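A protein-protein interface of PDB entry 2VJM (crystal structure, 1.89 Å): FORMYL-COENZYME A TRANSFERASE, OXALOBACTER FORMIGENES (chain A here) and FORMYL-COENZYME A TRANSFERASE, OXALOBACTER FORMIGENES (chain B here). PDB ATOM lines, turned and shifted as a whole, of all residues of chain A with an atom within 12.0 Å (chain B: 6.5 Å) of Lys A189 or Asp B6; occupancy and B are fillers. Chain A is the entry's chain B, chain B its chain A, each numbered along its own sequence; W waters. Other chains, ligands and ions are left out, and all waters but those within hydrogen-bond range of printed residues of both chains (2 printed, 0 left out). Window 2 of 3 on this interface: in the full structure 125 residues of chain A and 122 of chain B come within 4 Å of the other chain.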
ATOM      1  N   PRO A 117      13.039   2.563 -27.306  1.00  0.00           N
ATOM      2  CA  PRO A 117      13.582   1.291 -27.806  1.00  0.00           C
ATOM      3  C   PRO A 117      13.258   0.062 -26.950  1.00  0.00           C
ATOM      4  O   PRO A 117      13.425  -1.065 -27.418  1.00  0.00           O
ATOM      5  CB  PRO A 117      15.102   1.528 -27.813  1.00  0.00           C
ATOM      6  CG  PRO A 117      15.284   2.996 -27.707  1.00  0.00           C
ATOM      7  CD  PRO A 117      14.108   3.515 -26.957  1.00  0.00           C
ATOM      8  N   ARG A 118      12.820   0.275 -25.710  1.00  0.00           N
ATOM      9  CA  ARG A 118      12.490  -0.821 -24.806  1.00  0.00           C
ATOM     10  C   ARG A 118      11.014  -1.238 -24.822  1.00  0.00           C
ATOM     11  O   ARG A 118      10.679  -2.303 -24.307  1.00  0.00           O
ATOM     12  CB  ARG A 118      12.886  -0.452 -23.379  1.00  0.00           C
ATOM     13  CG  ARG A 118      14.398  -0.347 -23.169  1.00  0.00           C
ATOM     14  CD  ARG A 118      14.746  -0.058 -21.713  1.00  0.00           C
ATOM     15  NE  ARG A 118      14.126  -1.017 -20.803  1.00  0.00           N
ATOM     16  CZ  ARG A 118      14.545  -2.265 -20.604  1.00  0.00           C
ATOM     17  NH1 ARG A 118      15.607  -2.752 -21.240  1.00  0.00           N
ATOM     18  NH2 ARG A 118      13.885  -3.043 -19.762  1.00  0.00           N
ATOM     19  N   ILE A 120       7.286  -2.575 -25.767  1.00  0.00           N
ATOM     20  CA  ILE A 120       6.695  -3.667 -26.537  1.00  0.00           C
ATOM     21  C   ILE A 120       5.324  -3.190 -27.030  1.00  0.00           C
ATOM     22  O   ILE A 120       4.553  -2.623 -26.257  1.00  0.00           O
ATOM     23  CB  ILE A 120       6.550  -4.946 -25.660  1.00  0.00           C
ATOM     24  CG1 ILE A 120       7.931  -5.489 -25.267  1.00  0.00           C
ATOM     25  CG2 ILE A 120       5.725  -6.030 -26.384  1.00  0.00           C
ATOM     26  CD1 ILE A 120       7.944  -6.238 -23.942  1.00  0.00           C
ATOM     27  N   ILE A 180       3.092 -11.099 -25.094  1.00  0.00           N
ATOM     28  CA  ILE A 180       3.675  -9.993 -24.328  1.00  0.00           C
ATOM     29  C   ILE A 180       4.716 -10.489 -23.321  1.00  0.00           C
ATOM     30  O   ILE A 180       5.834  -9.958 -23.258  1.00  0.00           O
ATOM     31  CB  ILE A 180       2.581  -9.185 -23.591  1.00  0.00           C
ATOM     32  CG1 ILE A 180       1.705  -8.431 -24.601  1.00  0.00           C
ATOM     33  CG2 ILE A 180       3.211  -8.205 -22.591  1.00  0.00           C
ATOM     34  CD1 ILE A 180       0.410  -7.895 -24.016  1.00  0.00           C
ATOM     35  N   LEU A 181       4.350 -11.506 -22.544  1.00  0.00           N
ATOM     36  CA  LEU A 181       5.268 -12.084 -21.561  1.00  0.00           C
ATOM     37  C   LEU A 181       6.501 -12.682 -22.246  1.00  0.00           C
ATOM     38  O   LEU A 181       7.627 -12.523 -21.757  1.00  0.00           O
ATOM     39  CB  LEU A 181       4.553 -13.115 -20.680  1.00  0.00           C
ATOM     40  CG  LEU A 181       3.478 -12.546 -19.749  1.00  0.00           C
ATOM     41  CD1 LEU A 181       2.722 -13.651 -19.038  1.00  0.00           C
ATOM     42  CD2 LEU A 181       4.082 -11.565 -18.729  1.00  0.00           C
ATOM     43  N   ALA A 182       6.296 -13.337 -23.388  1.00  0.00           N
ATOM     44  CA  ALA A 182       7.404 -13.819 -24.217  1.00  0.00           C
ATOM     45  C   ALA A 182       8.329 -12.666 -24.642  1.00  0.00           C
ATOM     46  O   ALA A 182       9.554 -12.797 -24.593  1.00  0.00           O
ATOM     47  CB  ALA A 182       6.880 -14.566 -25.433  1.00  0.00           C
ATOM     48  N   ALA A 183       7.740 -11.535 -25.030  1.00  0.00           N
ATOM     49  CA  ALA A 183       8.504 -10.346 -25.429  1.00  0.00           C
ATOM     50  C   ALA A 183       9.289  -9.734 -24.261  1.00  0.00           C
ATOM     51  O   ALA A 183      10.400  -9.219 -24.457  1.00  0.00           O
ATOM     52  CB  ALA A 183       7.581  -9.305 -26.053  1.00  0.00           C
ATOM     53  N   LEU A 184       8.720  -9.796 -23.058  1.00  0.00           N
ATOM     54  CA  LEU A 184       9.433  -9.368 -21.843  1.00  0.00           C
ATOM     55  C   LEU A 184      10.620 -10.286 -21.540  1.00  0.00           C
ATOM     56  O   LEU A 184      11.674  -9.815 -21.090  1.00  0.00           O
ATOM     57  CB  LEU A 184       8.495  -9.317 -20.632  1.00  0.00           C
ATOM     58  CG  LEU A 184       7.464  -8.187 -20.583  1.00  0.00           C
ATOM     59  CD1 LEU A 184       6.473  -8.422 -19.447  1.00  0.00           C
ATOM     60  CD2 LEU A 184       8.142  -6.818 -20.445  1.00  0.00           C
ATOM     61  N   GLU A 185      10.447 -11.586 -21.779  1.00  0.00           N
ATOM     62  CA  GLU A 185      11.533 -12.555 -21.600  1.00  0.00           C
ATOM     63  C   GLU A 185      12.725 -12.237 -22.488  1.00  0.00           C
ATOM     64  O   GLU A 185      13.860 -12.214 -22.013  1.00  0.00           O
ATOM     65  CB  GLU A 185      11.074 -13.998 -21.870  1.00  0.00           C
ATOM     66  CG  GLU A 185      10.903 -14.871 -20.639  1.00  0.00           C
ATOM     67  CD  GLU A 185      12.133 -14.895 -19.722  1.00  0.00           C
ATOM     68  OE1 GLU A 185      12.154 -14.112 -18.756  1.00  0.00           O
ATOM     69  OE2 GLU A 185      13.069 -15.688 -19.957  1.00  0.00           O
ATOM     70  N   ILE A 186      12.470 -11.995 -23.769  1.00  0.00           N
ATOM     71  CA  ILE A 186      13.550 -11.734 -24.716  1.00  0.00           C
ATOM     72  C   ILE A 186      14.196 -10.357 -24.492  1.00  0.00           C
ATOM     73  O   ILE A 186      15.385 -10.178 -24.766  1.00  0.00           O
ATOM     74  CB  ILE A 186      13.083 -11.892 -26.189  1.00  0.00           C
ATOM     75  CG1 ILE A 186      14.290 -12.219 -27.089  1.00  0.00           C
ATOM     76  CG2 ILE A 186      12.335 -10.657 -26.671  1.00  0.00           C
ATOM     77  CD1 ILE A 186      13.947 -12.381 -28.564  1.00  0.00           C
ATOM     78  N   ARG A 187      13.418  -9.399 -23.982  1.00  0.00           N
ATOM     79  CA  ARG A 187      13.937  -8.067 -23.681  1.00  0.00           C
ATOM     80  C   ARG A 187      15.027  -8.120 -22.602  1.00  0.00           C
ATOM     81  O   ARG A 187      15.974  -7.330 -22.642  1.00  0.00           O
ATOM     82  CB  ARG A 187      12.809  -7.114 -23.268  1.00  0.00           C
ATOM     83  CG  ARG A 187      13.244  -5.660 -23.177  1.00  0.00           C
ATOM     84  CD  ARG A 187      12.096  -4.729 -22.845  1.00  0.00           C
ATOM     85  NE  ARG A 187      11.579  -4.947 -21.493  1.00  0.00           N
ATOM     86  CZ  ARG A 187      10.819  -4.085 -20.822  1.00  0.00           C
ATOM     87  NH1 ARG A 187      10.483  -2.918 -21.349  1.00  0.00           N
ATOM     88  NH2 ARG A 187      10.406  -4.392 -19.601  1.00  0.00           N
ATOM     89  N   HIS A 188      14.908  -9.051 -21.656  1.00  0.00           N
ATOM     90  CA  HIS A 188      15.985  -9.290 -20.686  1.00  0.00           C
ATOM     91  C   HIS A 188      17.309  -9.631 -21.384  1.00  0.00           C
ATOM     92  O   HIS A 188      18.372  -9.294 -20.878  1.00  0.00           O
ATOM     93  CB  HIS A 188      15.624 -10.403 -19.700  1.00  0.00           C
ATOM     94  CG  HIS A 188      14.584 -10.013 -18.697  1.00  0.00           C
ATOM     95  ND1 HIS A 188      14.823  -9.102 -17.691  1.00  0.00           N
ATOM     96  CD2 HIS A 188      13.303 -10.422 -18.537  1.00  0.00           C
ATOM     97  CE1 HIS A 188      13.731  -8.959 -16.961  1.00  0.00           C
ATOM     98  NE2 HIS A 188      12.794  -9.750 -17.452  1.00  0.00           N
ATOM     99  N   LYS A 189      17.231 -10.280 -22.546  1.00  0.00           N
ATOM    100  CA  LYS A 189      18.417 -10.668 -23.316  1.00  0.00           C
ATOM    101  C   LYS A 189      18.906  -9.532 -24.219  1.00  0.00           C
ATOM    102  O   LYS A 189      20.093  -9.196 -24.220  1.00  0.00           O
ATOM    103  CB  LYS A 189      18.114 -11.903 -24.179  1.00  0.00           C
ATOM    104  CG  LYS A 189      17.480 -13.066 -23.408  1.00  0.00           C
ATOM    105  CD  LYS A 189      16.709 -14.031 -24.314  1.00  0.00           C
ATOM    106  CE  LYS A 189      17.344 -15.412 -24.333  1.00  0.00           C
ATOM    107  NZ  LYS A 189      16.699 -16.287 -25.346  1.00  0.00           N
ATOM    108  N   THR A 190      17.983  -8.940 -24.976  1.00  0.00           N
ATOM    109  CA  THR A 190      18.331  -7.990 -26.036  1.00  0.00           C
ATOM    110  C   THR A 190      18.324  -6.522 -25.600  1.00  0.00           C
ATOM    111  O   THR A 190      18.936  -5.680 -26.256  1.00  0.00           O
ATOM    112  CB  THR A 190      17.358  -8.117 -27.228  1.00  0.00           C
ATOM    113  OG1 THR A 190      16.065  -7.641 -26.838  1.00  0.00           O
ATOM    114  CG2 THR A 190      17.256  -9.568 -27.691  1.00  0.00           C
ATOM    115  N   GLY A 191      17.611  -6.215 -24.520  1.00  0.00           N
ATOM    116  CA  GLY A 191      17.382  -4.830 -24.106  1.00  0.00           C
ATOM    117  C   GLY A 191      16.433  -4.057 -25.014  1.00  0.00           C
ATOM    118  O   GLY A 191      16.302  -2.842 -24.883  1.00  0.00           O
ATOM    119  N   ARG A 192      15.761  -4.758 -25.929  1.00  0.00           N
ATOM    120  CA  ARG A 192      14.902  -4.116 -26.917  1.00  0.00           C
ATOM    121  C   ARG A 192      13.492  -4.703 -26.888  1.00  0.00           C
ATOM    122  O   ARG A 192      13.308  -5.903 -26.649  1.00  0.00           O
ATOM    123  CB  ARG A 192      15.492  -4.274 -28.319  1.00  0.00           C
ATOM    124  CG  ARG A 192      16.789  -3.494 -28.566  1.00  0.00           C
ATOM    125  CD  ARG A 192      16.573  -1.989 -28.525  1.00  0.00           C
ATOM    126  NE  ARG A 192      15.605  -1.531 -29.526  1.00  0.00           N
ATOM    127  CZ  ARG A 192      15.899  -1.187 -30.780  1.00  0.00           C
ATOM    128  NH1 ARG A 192      17.148  -1.244 -31.238  1.00  0.00           N
ATOM    129  NH2 ARG A 192      14.930  -0.784 -31.592  1.00  0.00           N
ATOM    130  N   GLY A 193      12.508  -3.840 -27.129  1.00  0.00           N
ATOM    131  CA  GLY A 193      11.118  -4.255 -27.246  1.00  0.00           C
ATOM    132  C   GLY A 193      10.857  -4.835 -28.624  1.00  0.00           C
ATOM    133  O   GLY A 193      11.637  -4.626 -29.552  1.00  0.00           O
ATOM    134  N   GLN A 194       9.762  -5.574 -28.751  1.00  0.00           N
ATOM    135  CA  GLN A 194       9.350  -6.137 -30.029  1.00  0.00           C
ATOM    136  C   GLN A 194       7.881  -5.816 -30.270  1.00  0.00           C
ATOM    137  O   GLN A 194       7.172  -5.381 -29.357  1.00  0.00           O
ATOM    138  CB  GLN A 194       9.574  -7.657 -30.055  1.00  0.00           C
ATOM    139  CG  GLN A 194      11.028  -8.074 -30.305  1.00  0.00           C
ATOM    140  CD  GLN A 194      11.176  -9.526 -30.735  1.00  0.00           C
ATOM    141  OE1 GLN A 194      10.292 -10.097 -31.368  1.00  0.00           O
ATOM    142  NE2 GLN A 194      12.322 -10.124 -30.405  1.00  0.00           N
ATOM    143  N   THR B   2      17.577 -14.635 -29.297  1.00  0.00           N
ATOM    144  CA  THR B   2      16.966 -14.463 -30.655  1.00  0.00           C
ATOM    145  C   THR B   2      15.532 -15.005 -30.704  1.00  0.00           C
ATOM    146  O   THR B   2      14.665 -14.391 -31.325  1.00  0.00           O
ATOM    147  CB  THR B   2      17.829 -15.122 -31.741  1.00  0.00           C
ATOM    148  OG1 THR B   2      19.105 -14.468 -31.789  1.00  0.00           O
ATOM    149  CG2 THR B   2      17.164 -15.017 -33.112  1.00  0.00           C
ATOM    150  N   LYS B   3      15.288 -16.152 -30.069  1.00  0.00           N
ATOM    151  CA  LYS B   3      13.919 -16.564 -29.738  1.00  0.00           C
ATOM    152  C   LYS B   3      13.725 -16.396 -28.225  1.00  0.00           C
ATOM    153  O   LYS B   3      14.674 -16.581 -27.458  1.00  0.00           O
ATOM    154  CB  LYS B   3      13.620 -18.004 -30.164  1.00  0.00           C
ATOM    155  CG  LYS B   3      13.877 -18.315 -31.643  1.00  0.00           C
ATOM    156  CD  LYS B   3      13.232 -19.650 -32.032  1.00  0.00           C
ATOM    157  CE  LYS B   3      13.780 -20.217 -33.345  1.00  0.00           C
ATOM    158  NZ  LYS B   3      13.135 -19.608 -34.531  1.00  0.00           N
ATOM    159  N   PRO B   4      12.499 -16.029 -27.793  1.00  0.00           N
ATOM    160  CA  PRO B   4      12.204 -15.694 -26.394  1.00  0.00           C
ATOM    161  C   PRO B   4      12.665 -16.710 -25.363  1.00  0.00           C
ATOM    162  O   PRO B   4      13.134 -16.320 -24.296  1.00  0.00           O
ATOM    163  CB  PRO B   4      10.674 -15.593 -26.376  1.00  0.00           C
ATOM    164  CG  PRO B   4      10.322 -15.170 -27.738  1.00  0.00           C
ATOM    165  CD  PRO B   4      11.300 -15.883 -28.638  1.00  0.00           C
ATOM    166  N   LEU B   5      12.525 -17.997 -25.672  1.00  0.00           N
ATOM    167  CA  LEU B   5      12.819 -19.047 -24.705  1.00  0.00           C
ATOM    168  C   LEU B   5      14.076 -19.850 -25.047  1.00  0.00           C
ATOM    169  O   LEU B   5      14.310 -20.916 -24.470  1.00  0.00           O
ATOM    170  CB  LEU B   5      11.607 -19.969 -24.550  1.00  0.00           C
ATOM    171  CG  LEU B   5      10.284 -19.260 -24.222  1.00  0.00           C
ATOM    172  CD1 LEU B   5       9.160 -20.267 -24.069  1.00  0.00           C
ATOM    173  CD2 LEU B   5      10.408 -18.403 -22.967  1.00  0.00           C
ATOM    174  N   ASP B   6      14.893 -19.340 -25.966  1.00  0.00           N
ATOM    175  CA  ASP B   6      16.215 -19.931 -26.203  1.00  0.00           C
ATOM    176  C   ASP B   6      16.950 -20.042 -24.877  1.00  0.00           C
ATOM    177  O   ASP B   6      16.979 -19.086 -24.110  1.00  0.00           O
ATOM    178  CB  ASP B   6      17.038 -19.092 -27.187  1.00  0.00           C
ATOM    179  CG  ASP B   6      16.630 -19.315 -28.626  1.00  0.00           C
ATOM    180  OD1 ASP B   6      15.902 -20.301 -28.903  1.00  0.00           O
ATOM    181  OD2 ASP B   6      17.038 -18.502 -29.483  1.00  0.00           O
ATOM    182  N   GLY B   7      17.498 -21.222 -24.597  1.00  0.00           N
ATOM    183  CA  GLY B   7      18.219 -21.466 -23.351  1.00  0.00           C
ATOM    184  C   GLY B   7      17.363 -21.940 -22.189  1.00  0.00           C
ATOM    185  O   GLY B   7      17.901 -22.366 -21.165  1.00  0.00           O
ATOM    186  N   ILE B   8      16.036 -21.876 -22.327  1.00  0.00           N
ATOM    187  CA  ILE B   8      15.135 -22.342 -21.274  1.00  0.00           C
ATOM    188  C   ILE B   8      15.003 -23.854 -21.375  1.00  0.00           C
ATOM    189  O   ILE B   8      14.583 -24.381 -22.402  1.00  0.00           O
ATOM    190  CB  ILE B   8      13.726 -21.675 -21.359  1.00  0.00           C
ATOM    191  CG1 ILE B   8      13.824 -20.172 -21.089  1.00  0.00           C
ATOM    192  CG2 ILE B   8      12.753 -22.315 -20.367  1.00  0.00           C
ATOM    193  CD1 ILE B   8      14.294 -19.826 -19.685  1.00  0.00           C
ATOM    194  N   LEU B  29       8.696 -21.331 -29.356  1.00  0.00           N
ATOM    195  CA  LEU B  29       9.333 -20.064 -28.997  1.00  0.00           C
ATOM    196  C   LEU B  29      10.791 -20.221 -28.526  1.00  0.00           C
ATOM    197  O   LEU B  29      11.364 -19.275 -27.970  1.00  0.00           O
ATOM    198  CB  LEU B  29       8.511 -19.331 -27.925  1.00  0.00           C
ATOM    199  CG  LEU B  29       7.068 -18.936 -28.285  1.00  0.00           C
ATOM    200  CD1 LEU B  29       6.568 -17.844 -27.358  1.00  0.00           C
ATOM    201  CD2 LEU B  29       6.945 -18.494 -29.733  1.00  0.00           C
ATOM    202  N   GLY B  30      11.375 -21.400 -28.746  1.00  0.00           N
ATOM    203  CA  GLY B  30      12.816 -21.619 -28.544  1.00  0.00           C
ATOM    204  C   GLY B  30      13.234 -22.533 -27.405  1.00  0.00           C
ATOM    205  O   GLY B  30      14.420 -22.852 -27.278  1.00  0.00           O
ATOM    206  N   ALA B  31      12.289 -22.966 -26.572  1.00  0.00           N
ATOM    207  CA  ALA B  31      12.633 -23.776 -25.398  1.00  0.00           C
ATOM    208  C   ALA B  31      13.196 -25.155 -25.767  1.00  0.00           C
ATOM    209  O   ALA B  31      12.806 -25.756 -26.778  1.00  0.00           O
ATOM    210  CB  ALA B  31      11.430 -23.939 -24.472  1.00  0.00           C
ATOM    211  N   ASN B  32      14.122 -25.613 -24.926  1.00  0.00           N
ATOM    212  CA  ASN B  32      14.705 -26.955 -25.007  1.00  0.00           C
ATOM    213  C   ASN B  32      13.817 -27.916 -24.215  1.00  0.00           C
ATOM    214  O   ASN B  32      13.925 -28.007 -22.983  1.00  0.00           O
ATOM    215  CB  ASN B  32      16.145 -26.927 -24.454  1.00  0.00           C
ATOM    216  CG  ASN B  32      16.793 -28.313 -24.358  1.00  0.00           C
ATOM    217  OD1 ASN B  32      17.658 -28.538 -23.509  1.00  0.00           O
ATOM    218  ND2 ASN B  32      16.393 -29.229 -25.228  1.00  0.00           N
HETATM  219  O   HOH W   1      14.020 -11.873 -31.723  1.00  0.00           O
HETATM  220  O   HOH W   2      14.746 -16.660 -21.860  1.00  0.00           O
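The backbone NH (N) of Leu B5 is in hydrogen-bond range of the backbone carbonyl oxygen (O) of Leu B29. The backbone carbonyl oxygen (O) of Ile A186 sits at hydrogen-bond distance from the side-chain hydroxyl (OG1) of Thr A190, at 3.3 Å. The backbone NH (N) of Lys B3 sits at hydrogen-bond distance from the side-chain carboxylate (OD2) of Asp B6.
Ile A180 touches none of the printed residues of chain B. Printed residues of chain B within 4 Å of Ala A182: Pro B4 and Leu B29. Of the printed residues of chain B, Glu A185 touches Pro B4. Of the printed residues of chain B, Ile A186 touches Thr B2 (3.5 Å) and Pro B4 (3.9 Å). Lys A189 touches just these residues of chain B: Lys B3, Pro B4 and Asp B6. Pro B4 touches just these residues of chain A: Ala A182, Glu A185, Ile A186 and Lys A189. No residue of chain A comes within 4 Å of Leu B5. Of the printed residues of chain A, Asp B6 touches Lys A189 (3.1 Å). No residue of chain A comes within 4 Å of Gly B7. No residue of chain A comes within 4 Å of Ile B8. No residue of chain A comes within 4 Å of Gly B30. No residue of chain A comes within 4 Å of Ala B31. The nearest residue of chain A that does not touch Asp B6 is Glu A185 (6.6 Å). The nearest printed residue of chain B that does not touch Glu A185 is Leu B5 (4.3 Å).
Ala A182 touches Pro B4. Ala A182 touches Leu B29 (CB to CD1, 3.8 Å). O of Pro B4 touches CB of Glu A185, at 3.9 Å. Thr B2 touches Ile A186. Pro B4 touches Ile A186 (CA to CB, 3.9 Å). NZ of Lys A189 touches O of Pro B4 (3.7 Å).
The backbone carbonyl oxygen (O) of Asp B6 sits at hydrogen-bond distance from the side-chain amino group (NZ) of Lys A189, at 3.1 Å. O of Lys B3 sits at hydrogen-bond distance from NZ of Lys A189, at 2.9 Å.
Of the 11 printed residues of chain B, 5 touch a printed residue of chain A. Printed residues of chain B that touch a printed residue of chain A: Thr B2, Lys B3, Pro B4, Asp B6 and Leu B29. Hydrophobic or aromatic side chains of chain B within 4 Å of the printed part of chain A: Pro B4 and Leu B29. Of the 18 printed residues of chain A, 4 touch a printed residue of chain B. Hydrophobic or aromatic side chains of chain A within 4 Å of the printed part of chain B: Ala A182 and Ile A186. Among the printed residues, no Asp or Glu carboxylate lies within 4 Å of a Lys or Arg side-chain nitrogen of the other chain.
Water W1 lies within hydrogen-bond range of the backbone carbonyl oxygen of Thr B2 (2.6 Å) and the side-chain amide nitrogen of Gln A194 (2.8 Å). Water W2 bridges the side-chain carboxylate (OE2) of Glu A185 (2.7 Å) and the backbone carbonyl oxygen (O) of Pro B4 (2.9 Å).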
